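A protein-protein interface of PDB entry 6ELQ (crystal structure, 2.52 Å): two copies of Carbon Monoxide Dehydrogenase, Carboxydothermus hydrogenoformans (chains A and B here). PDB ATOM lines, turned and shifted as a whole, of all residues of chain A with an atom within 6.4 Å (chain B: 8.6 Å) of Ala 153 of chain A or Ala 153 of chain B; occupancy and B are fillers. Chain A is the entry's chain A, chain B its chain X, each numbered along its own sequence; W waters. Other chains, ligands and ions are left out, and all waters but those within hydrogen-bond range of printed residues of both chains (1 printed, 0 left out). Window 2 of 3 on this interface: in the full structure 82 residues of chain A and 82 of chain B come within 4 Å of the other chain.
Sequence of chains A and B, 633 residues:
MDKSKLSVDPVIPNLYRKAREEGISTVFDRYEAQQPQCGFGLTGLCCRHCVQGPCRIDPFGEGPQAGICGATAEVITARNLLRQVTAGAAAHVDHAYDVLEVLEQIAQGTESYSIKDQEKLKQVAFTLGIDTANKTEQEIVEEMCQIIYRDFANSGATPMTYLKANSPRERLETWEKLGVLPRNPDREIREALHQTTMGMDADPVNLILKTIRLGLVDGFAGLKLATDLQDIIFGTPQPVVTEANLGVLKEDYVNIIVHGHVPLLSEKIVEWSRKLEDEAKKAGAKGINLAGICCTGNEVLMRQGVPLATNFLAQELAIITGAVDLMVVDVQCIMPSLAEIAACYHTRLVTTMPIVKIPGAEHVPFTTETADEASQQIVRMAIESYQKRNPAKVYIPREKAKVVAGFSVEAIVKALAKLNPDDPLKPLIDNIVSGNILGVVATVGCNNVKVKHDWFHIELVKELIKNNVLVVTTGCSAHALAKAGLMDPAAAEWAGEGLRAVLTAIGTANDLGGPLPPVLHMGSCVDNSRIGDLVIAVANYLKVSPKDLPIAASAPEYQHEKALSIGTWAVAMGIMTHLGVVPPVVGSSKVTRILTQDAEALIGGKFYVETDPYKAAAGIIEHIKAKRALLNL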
ATOM      1  N   TYR A  97      17.408   9.225  11.604  1.00  0.00           N
ATOM      2  CA  TYR A  97      16.726  10.280  10.866  1.00  0.00           C
ATOM      3  C   TYR A  97      15.212  10.160  10.972  1.00  0.00           C
ATOM      4  O   TYR A  97      14.510  11.174  10.925  1.00  0.00           O
ATOM      5  CB  TYR A  97      17.159  10.245   9.398  1.00  0.00           C
ATOM      6  CG  TYR A  97      16.818  11.482   8.604  1.00  0.00           C
ATOM      7  CD1 TYR A  97      17.635  12.604   8.648  1.00  0.00           C
ATOM      8  CD2 TYR A  97      15.693  11.521   7.792  1.00  0.00           C
ATOM      9  CE1 TYR A  97      17.335  13.734   7.914  1.00  0.00           C
ATOM     10  CE2 TYR A  97      15.385  12.646   7.057  1.00  0.00           C
ATOM     11  CZ  TYR A  97      16.209  13.748   7.122  1.00  0.00           C
ATOM     12  OH  TYR A  97      15.908  14.869   6.388  1.00  0.00           O
ATOM     13  N   ILE A 148      20.260  19.769  14.479  1.00  0.00           N
ATOM     14  CA  ILE A 148      20.511  18.441  13.929  1.00  0.00           C
ATOM     15  C   ILE A 148      20.336  18.439  12.416  1.00  0.00           C
ATOM     16  O   ILE A 148      21.169  17.892  11.685  1.00  0.00           O
ATOM     17  CB  ILE A 148      19.602  17.396  14.602  1.00  0.00           C
ATOM     18  CG1 ILE A 148      19.785  17.430  16.119  1.00  0.00           C
ATOM     19  CG2 ILE A 148      19.917  16.009  14.069  1.00  0.00           C
ATOM     20  CD1 ILE A 148      18.870  16.484  16.862  1.00  0.00           C
ATOM     21  N   TYR A 149      19.253  19.045  11.920  1.00  0.00           N
ATOM     22  CA  TYR A 149      19.057  19.132  10.476  1.00  0.00           C
ATOM     23  C   TYR A 149      20.174  19.909   9.797  1.00  0.00           C
ATOM     24  O   TYR A 149      20.429  19.696   8.606  1.00  0.00           O
ATOM     25  CB  TYR A 149      17.708  19.773  10.148  1.00  0.00           C
ATOM     26  CG  TYR A 149      16.530  18.829  10.262  1.00  0.00           C
ATOM     27  CD1 TYR A 149      16.333  17.818   9.328  1.00  0.00           C
ATOM     28  CD2 TYR A 149      15.610  18.954  11.297  1.00  0.00           C
ATOM     29  CE1 TYR A 149      15.257  16.954   9.427  1.00  0.00           C
ATOM     30  CE2 TYR A 149      14.533  18.096  11.405  1.00  0.00           C
ATOM     31  CZ  TYR A 149      14.360  17.098  10.468  1.00  0.00           C
ATOM     32  OH  TYR A 149      13.285  16.243  10.574  1.00  0.00           O
ATOM     33  N   ARG A 150      20.847  20.803  10.526  1.00  0.00           N
ATOM     34  CA  ARG A 150      22.004  21.486   9.962  1.00  0.00           C
ATOM     35  C   ARG A 150      23.119  20.500   9.638  1.00  0.00           C
ATOM     36  O   ARG A 150      23.810  20.647   8.624  1.00  0.00           O
ATOM     37  CB  ARG A 150      22.501  22.569  10.919  1.00  0.00           C
ATOM     38  CG  ARG A 150      21.879  23.933  10.671  1.00  0.00           C
ATOM     39  CD  ARG A 150      22.588  25.027  11.454  1.00  0.00           C
ATOM     40  NE  ARG A 150      22.177  25.060  12.854  1.00  0.00           N
ATOM     41  CZ  ARG A 150      21.154  25.774  13.313  1.00  0.00           C
ATOM     42  NH1 ARG A 150      20.436  26.516  12.480  1.00  0.00           N
ATOM     43  NH2 ARG A 150      20.846  25.746  14.602  1.00  0.00           N
ATOM     44  N   ASP A 151      23.305  19.483  10.486  1.00  0.00           N
ATOM     45  CA  ASP A 151      24.317  18.469  10.206  1.00  0.00           C
ATOM     46  C   ASP A 151      24.016  17.736   8.904  1.00  0.00           C
ATOM     47  O   ASP A 151      24.926  17.458   8.116  1.00  0.00           O
ATOM     48  CB  ASP A 151      24.416  17.481  11.369  1.00  0.00           C
ATOM     49  CG  ASP A 151      25.152  18.060  12.564  1.00  0.00           C
ATOM     50  OD1 ASP A 151      25.578  19.231  12.496  1.00  0.00           O
ATOM     51  OD2 ASP A 151      25.307  17.342  13.573  1.00  0.00           O
ATOM     52  N   PHE A 152      22.744  17.427   8.657  1.00  0.00           N
ATOM     53  CA  PHE A 152      22.329  16.826   7.396  1.00  0.00           C
ATOM     54  C   PHE A 152      22.285  17.828   6.248  1.00  0.00           C
ATOM     55  O   PHE A 152      21.933  17.446   5.127  1.00  0.00           O
ATOM     56  CB  PHE A 152      20.960  16.160   7.559  1.00  0.00           C
ATOM     57  CG  PHE A 152      20.990  14.914   8.398  1.00  0.00           C
ATOM     58  CD1 PHE A 152      20.924  14.990   9.781  1.00  0.00           C
ATOM     59  CD2 PHE A 152      21.087  13.665   7.804  1.00  0.00           C
ATOM     60  CE1 PHE A 152      20.955  13.843  10.554  1.00  0.00           C
ATOM     61  CE2 PHE A 152      21.118  12.517   8.571  1.00  0.00           C
ATOM     62  CZ  PHE A 152      21.052  12.607   9.948  1.00  0.00           C
ATOM     63  N   ALA A 153      22.633  19.092   6.500  1.00  0.00           N
ATOM     64  CA  ALA A 153      22.634  20.122   5.473  1.00  0.00           C
ATOM     65  C   ALA A 153      23.958  20.866   5.370  1.00  0.00           C
ATOM     66  O   ALA A 153      24.053  21.819   4.588  1.00  0.00           O
ATOM     67  CB  ALA A 153      21.511  21.136   5.731  1.00  0.00           C
ATOM     68  N   ASN A 154      24.971  20.464   6.130  1.00  0.00           N
ATOM     69  CA  ASN A 154      26.242  21.178   6.155  1.00  0.00           C
ATOM     70  C   ASN A 154      26.980  20.986   4.833  1.00  0.00           C
ATOM     71  O   ASN A 154      27.287  19.854   4.442  1.00  0.00           O
ATOM     72  CB  ASN A 154      27.087  20.680   7.325  1.00  0.00           C
ATOM     73  CG  ASN A 154      28.402  21.416   7.450  1.00  0.00           C
ATOM     74  OD1 ASN A 154      28.518  22.573   7.053  1.00  0.00           O
ATOM     75  ND2 ASN A 154      29.406  20.743   8.003  1.00  0.00           N
ATOM     76  N   SER A 155      27.265  22.091   4.145  1.00  0.00           N
ATOM     77  CA  SER A 155      28.018  22.062   2.898  1.00  0.00           C
ATOM     78  C   SER A 155      29.466  22.497   3.073  1.00  0.00           C
ATOM     79  O   SER A 155      30.203  22.564   2.084  1.00  0.00           O
ATOM     80  CB  SER A 155      27.342  22.948   1.847  1.00  0.00           C
ATOM     81  OG  SER A 155      27.522  24.320   2.147  1.00  0.00           O
ATOM     82  N   GLY A 156      29.891  22.795   4.302  1.00  0.00           N
ATOM     83  CA  GLY A 156      31.227  23.268   4.569  1.00  0.00           C
ATOM     84  C   GLY A 156      32.120  22.204   5.174  1.00  0.00           C
ATOM     85  O   GLY A 156      31.747  21.038   5.322  1.00  0.00           O
ATOM     86  N   ASN A 184      28.916  15.899   7.306  1.00  0.00           N
ATOM     87  CA  ASN A 184      27.513  15.742   6.961  1.00  0.00           C
ATOM     88  C   ASN A 184      27.285  14.258   6.732  1.00  0.00           C
ATOM     89  O   ASN A 184      27.873  13.681   5.807  1.00  0.00           O
ATOM     90  CB  ASN A 184      27.173  16.570   5.716  1.00  0.00           C
ATOM     91  CG  ASN A 184      25.714  16.453   5.292  1.00  0.00           C
ATOM     92  OD1 ASN A 184      25.088  15.401   5.414  1.00  0.00           O
ATOM     93  ND2 ASN A 184      25.173  17.547   4.773  1.00  0.00           N
ATOM     94  N   PRO A 185      26.461  13.601   7.553  1.00  0.00           N
ATOM     95  CA  PRO A 185      26.278  12.149   7.381  1.00  0.00           C
ATOM     96  C   PRO A 185      25.776  11.773   6.001  1.00  0.00           C
ATOM     97  O   PRO A 185      26.288  10.820   5.400  1.00  0.00           O
ATOM     98  CB  PRO A 185      25.270  11.789   8.484  1.00  0.00           C
ATOM     99  CG  PRO A 185      24.616  13.080   8.864  1.00  0.00           C
ATOM    100  CD  PRO A 185      25.652  14.141   8.658  1.00  0.00           C
ATOM    101  N   TYR B  97      27.798  18.116  -7.325  1.00  0.00           N
ATOM    102  CA  TYR B  97      27.982  18.854  -6.079  1.00  0.00           C
ATOM    103  C   TYR B  97      29.322  19.582  -6.062  1.00  0.00           C
ATOM    104  O   TYR B  97      29.430  20.688  -5.519  1.00  0.00           O
ATOM    105  CB  TYR B  97      27.872  17.890  -4.899  1.00  0.00           C
ATOM    106  CG  TYR B  97      27.682  18.542  -3.553  1.00  0.00           C
ATOM    107  CD1 TYR B  97      26.422  18.930  -3.120  1.00  0.00           C
ATOM    108  CD2 TYR B  97      28.760  18.744  -2.701  1.00  0.00           C
ATOM    109  CE1 TYR B  97      26.242  19.514  -1.883  1.00  0.00           C
ATOM    110  CE2 TYR B  97      28.591  19.327  -1.463  1.00  0.00           C
ATOM    111  CZ  TYR B  97      27.330  19.709  -1.059  1.00  0.00           C
ATOM    112  OH  TYR B  97      27.160  20.289   0.174  1.00  0.00           O
ATOM    113  N   GLU B 104      29.013  28.429  -5.767  1.00  0.00           N
ATOM    114  CA  GLU B 104      28.892  29.204  -4.538  1.00  0.00           C
ATOM    115  C   GLU B 104      30.152  30.017  -4.278  1.00  0.00           C
ATOM    116  O   GLU B 104      30.079  31.159  -3.808  1.00  0.00           O
ATOM    117  CB  GLU B 104      28.588  28.272  -3.366  1.00  0.00           C
ATOM    118  CG  GLU B 104      28.690  28.916  -1.997  1.00  0.00           C
ATOM    119  CD  GLU B 104      28.360  27.945  -0.880  1.00  0.00           C
ATOM    120  OE1 GLU B 104      27.167  27.831  -0.524  1.00  0.00           O
ATOM    121  OE2 GLU B 104      29.292  27.287  -0.371  1.00  0.00           O
ATOM    122  N   GLN B 146      21.292  28.924  -3.531  1.00  0.00           N
ATOM    123  CA  GLN B 146      20.383  28.688  -2.414  1.00  0.00           C
ATOM    124  C   GLN B 146      19.302  27.681  -2.783  1.00  0.00           C
ATOM    125  O   GLN B 146      18.955  26.810  -1.978  1.00  0.00           O
ATOM    126  CB  GLN B 146      19.758  30.008  -1.965  1.00  0.00           C
ATOM    127  CG  GLN B 146      20.755  30.987  -1.373  1.00  0.00           C
ATOM    128  CD  GLN B 146      20.181  32.380  -1.225  1.00  0.00           C
ATOM    129  OE1 GLN B 146      19.118  32.687  -1.767  1.00  0.00           O
ATOM    130  NE2 GLN B 146      20.883  33.235  -0.489  1.00  0.00           N
ATOM    131  N   ILE B 147      18.766  27.782  -4.000  1.00  0.00           N
ATOM    132  CA  ILE B 147      17.730  26.853  -4.441  1.00  0.00           C
ATOM    133  C   ILE B 147      18.290  25.441  -4.569  1.00  0.00           C
ATOM    134  O   ILE B 147      17.646  24.465  -4.167  1.00  0.00           O
ATOM    135  CB  ILE B 147      17.115  27.343  -5.766  1.00  0.00           C
ATOM    136  CG1 ILE B 147      16.400  28.679  -5.557  1.00  0.00           C
ATOM    137  CG2 ILE B 147      16.171  26.299  -6.345  1.00  0.00           C
ATOM    138  CD1 ILE B 147      15.805  29.255  -6.822  1.00  0.00           C
ATOM    139  N   ILE B 148      19.499  25.309  -5.115  1.00  0.00           N
ATOM    140  CA  ILE B 148      20.071  23.986  -5.342  1.00  0.00           C
ATOM    141  C   ILE B 148      20.466  23.334  -4.020  1.00  0.00           C
ATOM    142  O   ILE B 148      20.240  22.135  -3.814  1.00  0.00           O
ATOM    143  CB  ILE B 148      21.264  24.080  -6.310  1.00  0.00           C
ATOM    144  CG1 ILE B 148      20.812  24.654  -7.656  1.00  0.00           C
ATOM    145  CG2 ILE B 148      21.902  22.715  -6.508  1.00  0.00           C
ATOM    146  CD1 ILE B 148      21.954  25.035  -8.574  1.00  0.00           C
ATOM    147  N   TYR B 149      21.056  24.106  -3.103  1.00  0.00           N
ATOM    148  CA  TYR B 149      21.426  23.545  -1.807  1.00  0.00           C
ATOM    149  C   TYR B 149      20.203  23.116  -1.009  1.00  0.00           C
ATOM    150  O   TYR B 149      20.287  22.184  -0.200  1.00  0.00           O
ATOM    151  CB  TYR B 149      22.257  24.548  -1.005  1.00  0.00           C
ATOM    152  CG  TYR B 149      23.730  24.512  -1.337  1.00  0.00           C
ATOM    153  CD1 TYR B 149      24.501  23.398  -1.034  1.00  0.00           C
ATOM    154  CD2 TYR B 149      24.353  25.594  -1.946  1.00  0.00           C
ATOM    155  CE1 TYR B 149      25.846  23.358  -1.334  1.00  0.00           C
ATOM    156  CE2 TYR B 149      25.697  25.566  -2.249  1.00  0.00           C
ATOM    157  CZ  TYR B 149      26.441  24.447  -1.941  1.00  0.00           C
ATOM    158  OH  TYR B 149      27.782  24.419  -2.245  1.00  0.00           O
ATOM    159  N   ARG B 150      19.061  23.776  -1.218  1.00  0.00           N
ATOM    160  CA  ARG B 150      17.841  23.349  -0.545  1.00  0.00           C
ATOM    161  C   ARG B 150      17.393  21.967  -1.001  1.00  0.00           C
ATOM    162  O   ARG B 150      16.692  21.279  -0.252  1.00  0.00           O
ATOM    163  CB  ARG B 150      16.723  24.370  -0.763  1.00  0.00           C
ATOM    164  CG  ARG B 150      16.746  25.509   0.245  1.00  0.00           C
ATOM    165  CD  ARG B 150      15.438  26.280   0.258  1.00  0.00           C
ATOM    166  NE  ARG B 150      15.320  27.194  -0.874  1.00  0.00           N
ATOM    167  CZ  ARG B 150      15.776  28.442  -0.874  1.00  0.00           C
ATOM    168  NH1 ARG B 150      16.386  28.927   0.200  1.00  0.00           N
ATOM    169  NH2 ARG B 150      15.625  29.206  -1.946  1.00  0.00           N
ATOM    170  N   ASP B 151      17.785  21.542  -2.205  1.00  0.00           N
ATOM    171  CA  ASP B 151      17.525  20.166  -2.616  1.00  0.00           C
ATOM    172  C   ASP B 151      18.363  19.183  -1.807  1.00  0.00           C
ATOM    173  O   ASP B 151      17.889  18.098  -1.455  1.00  0.00           O
ATOM    174  CB  ASP B 151      17.795  19.998  -4.111  1.00  0.00           C
ATOM    175  CG  ASP B 151      16.647  20.496  -4.971  1.00  0.00           C
ATOM    176  OD1 ASP B 151      15.613  20.914  -4.412  1.00  0.00           O
ATOM    177  OD2 ASP B 151      16.777  20.465  -6.213  1.00  0.00           O
ATOM    178  N   PHE B 152      19.610  19.545  -1.502  1.00  0.00           N
ATOM    179  CA  PHE B 152      20.475  18.695  -0.694  1.00  0.00           C
ATOM    180  C   PHE B 152      20.171  18.790   0.793  1.00  0.00           C
ATOM    181  O   PHE B 152      20.766  18.043   1.578  1.00  0.00           O
ATOM    182  CB  PHE B 152      21.943  19.051  -0.940  1.00  0.00           C
ATOM    183  CG  PHE B 152      22.459  18.603  -2.280  1.00  0.00           C
ATOM    184  CD1 PHE B 152      22.272  19.385  -3.408  1.00  0.00           C
ATOM    185  CD2 PHE B 152      23.132  17.397  -2.410  1.00  0.00           C
ATOM    186  CE1 PHE B 152      22.744  18.974  -4.640  1.00  0.00           C
ATOM    187  CE2 PHE B 152      23.608  16.980  -3.638  1.00  0.00           C
ATOM    188  CZ  PHE B 152      23.413  17.770  -4.756  1.00  0.00           C
ATOM    189  N   ALA B 153      19.275  19.689   1.198  1.00  0.00           N
ATOM    190  CA  ALA B 153      18.881  19.834   2.592  1.00  0.00           C
ATOM    191  C   ALA B 153      17.410  19.522   2.823  1.00  0.00           C
ATOM    192  O   ALA B 153      16.960  19.548   3.975  1.00  0.00           O
ATOM    193  CB  ALA B 153      19.187  21.254   3.086  1.00  0.00           C
ATOM    194  N   ASN B 154      16.658  19.225   1.766  1.00  0.00           N
ATOM    195  CA  ASN B 154      15.225  18.987   1.883  1.00  0.00           C
ATOM    196  C   ASN B 154      14.946  17.775   2.763  1.00  0.00           C
ATOM    197  O   ASN B 154      15.465  16.682   2.521  1.00  0.00           O
ATOM    198  CB  ASN B 154      14.628  18.786   0.490  1.00  0.00           C
ATOM    199  CG  ASN B 154      13.134  18.572   0.521  1.00  0.00           C
ATOM    200  OD1 ASN B 154      12.452  18.992   1.455  1.00  0.00           O
ATOM    201  ND2 ASN B 154      12.612  17.917  -0.507  1.00  0.00           N
ATOM    202  N   SER B 155      14.117  17.972   3.789  1.00  0.00           N
ATOM    203  CA  SER B 155      13.743  16.902   4.702  1.00  0.00           C
ATOM    204  C   SER B 155      12.298  16.451   4.537  1.00  0.00           C
ATOM    205  O   SER B 155      11.890  15.480   5.185  1.00  0.00           O
ATOM    206  CB  SER B 155      13.980  17.335   6.154  1.00  0.00           C
ATOM    207  OG  SER B 155      13.111  18.387   6.529  1.00  0.00           O
ATOM    208  N   GLY B 156      11.520  17.114   3.681  1.00  0.00           N
ATOM    209  CA  GLY B 156      10.122  16.794   3.497  1.00  0.00           C
ATOM    210  C   GLY B 156       9.867  15.932   2.272  1.00  0.00           C
ATOM    211  O   GLY B 156      10.780  15.446   1.603  1.00  0.00           O
ATOM    212  N   MET B 160      12.596  17.230  -5.268  1.00  0.00           N
ATOM    213  CA  MET B 160      13.705  18.161  -5.424  1.00  0.00           C
ATOM    214  C   MET B 160      13.440  19.108  -6.584  1.00  0.00           C
ATOM    215  O   MET B 160      12.888  18.716  -7.618  1.00  0.00           O
ATOM    216  CB  MET B 160      15.020  17.412  -5.636  1.00  0.00           C
ATOM    217  CG  MET B 160      14.918  16.194  -6.524  1.00  0.00           C
ATOM    218  SD  MET B 160      16.544  15.484  -6.838  1.00  0.00           S
ATOM    219  CE  MET B 160      17.069  16.480  -8.225  1.00  0.00           C
ATOM    220  N   ARG B 183      13.227  13.256  -3.379  1.00  0.00           N
ATOM    221  CA  ARG B 183      13.044  14.434  -2.538  1.00  0.00           C
ATOM    222  C   ARG B 183      14.331  15.208  -2.310  1.00  0.00           C
ATOM    223  O   ARG B 183      14.314  16.442  -2.276  1.00  0.00           O
ATOM    224  CB  ARG B 183      12.472  14.025  -1.176  1.00  0.00           C
ATOM    225  CG  ARG B 183      11.159  13.268  -1.235  1.00  0.00           C
ATOM    226  CD  ARG B 183      10.978  12.412   0.009  1.00  0.00           C
ATOM    227  NE  ARG B 183      11.971  11.343   0.074  1.00  0.00           N
ATOM    228  CZ  ARG B 183      11.987  10.384   0.994  1.00  0.00           C
ATOM    229  NH1 ARG B 183      12.932   9.453   0.966  1.00  0.00           N
ATOM    230  NH2 ARG B 183      11.060  10.354   1.943  1.00  0.00           N
ATOM    231  N   ASN B 184      15.441  14.503  -2.152  1.00  0.00           N
ATOM    232  CA  ASN B 184      16.728  15.048  -1.748  1.00  0.00           C
ATOM    233  C   ASN B 184      17.777  14.019  -2.146  1.00  0.00           C
ATOM    234  O   ASN B 184      17.788  12.908  -1.603  1.00  0.00           O
ATOM    235  CB  ASN B 184      16.726  15.345  -0.243  1.00  0.00           C
ATOM    236  CG  ASN B 184      18.112  15.630   0.328  1.00  0.00           C
ATOM    237  OD1 ASN B 184      19.117  15.653  -0.382  1.00  0.00           O
ATOM    238  ND2 ASN B 184      18.160  15.862   1.635  1.00  0.00           N
ATOM    239  N   PRO B 185      18.665  14.351  -3.090  1.00  0.00           N
ATOM    240  CA  PRO B 185      19.567  13.317  -3.638  1.00  0.00           C
ATOM    241  C   PRO B 185      20.400  12.606  -2.585  1.00  0.00           C
ATOM    242  O   PRO B 185      20.480  11.371  -2.598  1.00  0.00           O
ATOM    243  CB  PRO B 185      20.435  14.106  -4.630  1.00  0.00           C
ATOM    244  CG  PRO B 185      20.260  15.549  -4.264  1.00  0.00           C
ATOM    245  CD  PRO B 185      18.873  15.665  -3.718  1.00  0.00           C
ATOM    246  N   ASP B 186      21.022  13.347  -1.667  1.00  0.00           N
ATOM    247  CA  ASP B 186      21.808  12.706  -0.616  1.00  0.00           C
ATOM    248  C   ASP B 186      20.936  11.825   0.271  1.00  0.00           C
ATOM    249  O   ASP B 186      21.366  10.747   0.701  1.00  0.00           O
ATOM    250  CB  ASP B 186      22.525  13.762   0.220  1.00  0.00           C
ATOM    251  CG  ASP B 186      23.750  14.313  -0.468  1.00  0.00           C
ATOM    252  OD1 ASP B 186      24.189  13.710  -1.469  1.00  0.00           O
ATOM    253  OD2 ASP B 186      24.278  15.344  -0.003  1.00  0.00           O
ATOM    254  N   ARG B 187      19.711  12.266   0.560  1.00  0.00           N
ATOM    255  CA  ARG B 187      18.828  11.470   1.406  1.00  0.00           C
ATOM    256  C   ARG B 187      18.373  10.203   0.691  1.00  0.00           C
ATOM    257  O   ARG B 187      18.260   9.141   1.313  1.00  0.00           O
ATOM    258  CB  ARG B 187      17.622  12.301   1.845  1.00  0.00           C
ATOM    259  CG  ARG B 187      16.750  11.616   2.880  1.00  0.00           C
ATOM    260  CD  ARG B 187      15.297  11.547   2.431  1.00  0.00           C
ATOM    261  NE  ARG B 187      14.450  10.892   3.425  1.00  0.00           N
ATOM    262  CZ  ARG B 187      13.600  11.530   4.221  1.00  0.00           C
ATOM    263  NH1 ARG B 187      12.875  10.848   5.099  1.00  0.00           N
ATOM    264  NH2 ARG B 187      13.470  12.847   4.139  1.00  0.00           N
ATOM    265  N   ARG B 190      21.169   7.674   0.781  1.00  0.00           N
ATOM    266  CA  ARG B 190      21.292   7.044   2.092  1.00  0.00           C
ATOM    267  C   ARG B 190      20.134   6.086   2.360  1.00  0.00           C
ATOM    268  O   ARG B 190      20.334   5.009   2.935  1.00  0.00           O
ATOM    269  CB  ARG B 190      21.375   8.114   3.182  1.00  0.00           C
ATOM    270  CG  ARG B 190      21.224   7.573   4.600  1.00  0.00           C
ATOM    271  CD  ARG B 190      19.921   8.045   5.230  1.00  0.00           C
ATOM    272  NE  ARG B 190      19.890   9.499   5.373  1.00  0.00           N
ATOM    273  CZ  ARG B 190      18.839  10.188   5.807  1.00  0.00           C
ATOM    274  NH1 ARG B 190      18.906  11.509   5.904  1.00  0.00           N
ATOM    275  NH2 ARG B 190      17.721   9.558   6.141  1.00  0.00           N
HETATM  276  O   HOH W   1      20.286  15.782   3.778  1.00  0.00           O
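Hydrophobic or aromatic side chains of chain A that line the printed part of chain B: Tyr 97, Tyr 149, Phe 152 and Ala 153.
Printed residues of chain B that touch a printed residue of chain A: Tyr 97, Tyr 149, Phe 152, Ala 153, Ser 155, Arg 187 and Arg 190.
Among the printed residues, no Asp or Glu carboxylate lies within 4 Å of a Lys or Arg side-chain nitrogen of the other chain.
Water W1 lies within hydrogen-bond range of O of Phe 152 of chain A (2.7 Å), ND2 of Asn 184 of chain B (3.0 Å) and O of Phe 152 of chain B (3.2 Å).
Of chain B, only Ala 153 (3.5 Å) comes within 4 Å of Ala 153 of chain A.
Ala 153 of chain B touches one residue of chain A.
Of the printed residues of chain A, Arg 190 of chain B touches Tyr 97 and Phe 152.
Printed residues of chain B within 4 Å of Tyr 149 of chain A: Ser 155 (3.5 Å).
Asp 186 of chain B touches none of the printed residues of chain A.
Gly 156 of chain A touches none of the printed residues of chain B.
The backbone carbonyl oxygen of Phe 152 of chain B lies within hydrogen-bond range of the side-chain amide nitrogen of Asn 184 of chain B (3.4 Å).
The backbone carbonyl oxygen of Ser 155 of chain B sits at hydrogen-bond distance from the guanidinium group of Arg 187 of chain B.
The backbone carbonyl oxygen of Phe 152 of chain A lies close to the side-chain amide nitrogen of Asn 184 of chain A (3.3 Å).
The side-chain amide nitrogen of Asn 184 of chain A lies close to the backbone NH of Ala 153 of chain A, 3.4 Å away.
Ser 155 of chain B touches Tyr 97 of chain A.
Arg 187 of chain B touches Tyr 97 of chain A (NH2 to CE2, 3.5 Å).
Arg 190 of chain B touches Tyr 97 of chain A (NH1 to CD1, 3.2 Å).
CB of Ser 155 of chain B touches CE1 of Tyr 149 of chain A, at 3.5 Å.
O of Phe 152 of chain B touches O of Phe 152 of chain A (3.8 Å).
Arg 190 of chain B touches Phe 152 of chain A.
Ala 153 of chain A touches Ala 153 of chain B (CB to CB, 3.5 Å).
Ser 155 of chain A touches Tyr 97 of chain B.
CE1 of Tyr 149 of chain B touches CB of Ser 155 of chain A (3.5 Å).
Tyr 97 of chain A touches Ser 155 of chain B, and with the chains exchanged Ser 155 of chain A touches Tyr 97 of chain B.
Tyr 149 of chain A touches Ser 155 of chain B, and with the chains exchanged Ser 155 of chain A touches Tyr 149 of chain B.
Phe 152 of chain B touches its own counterpart, Phe 152 of chain A.
Ala 153 of chain A touches its own counterpart, Ala 153 of chain B.
Of the 9 pairs that touch across the chains among the printed residues, 6 have their exchanged pair printed and touching as well.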
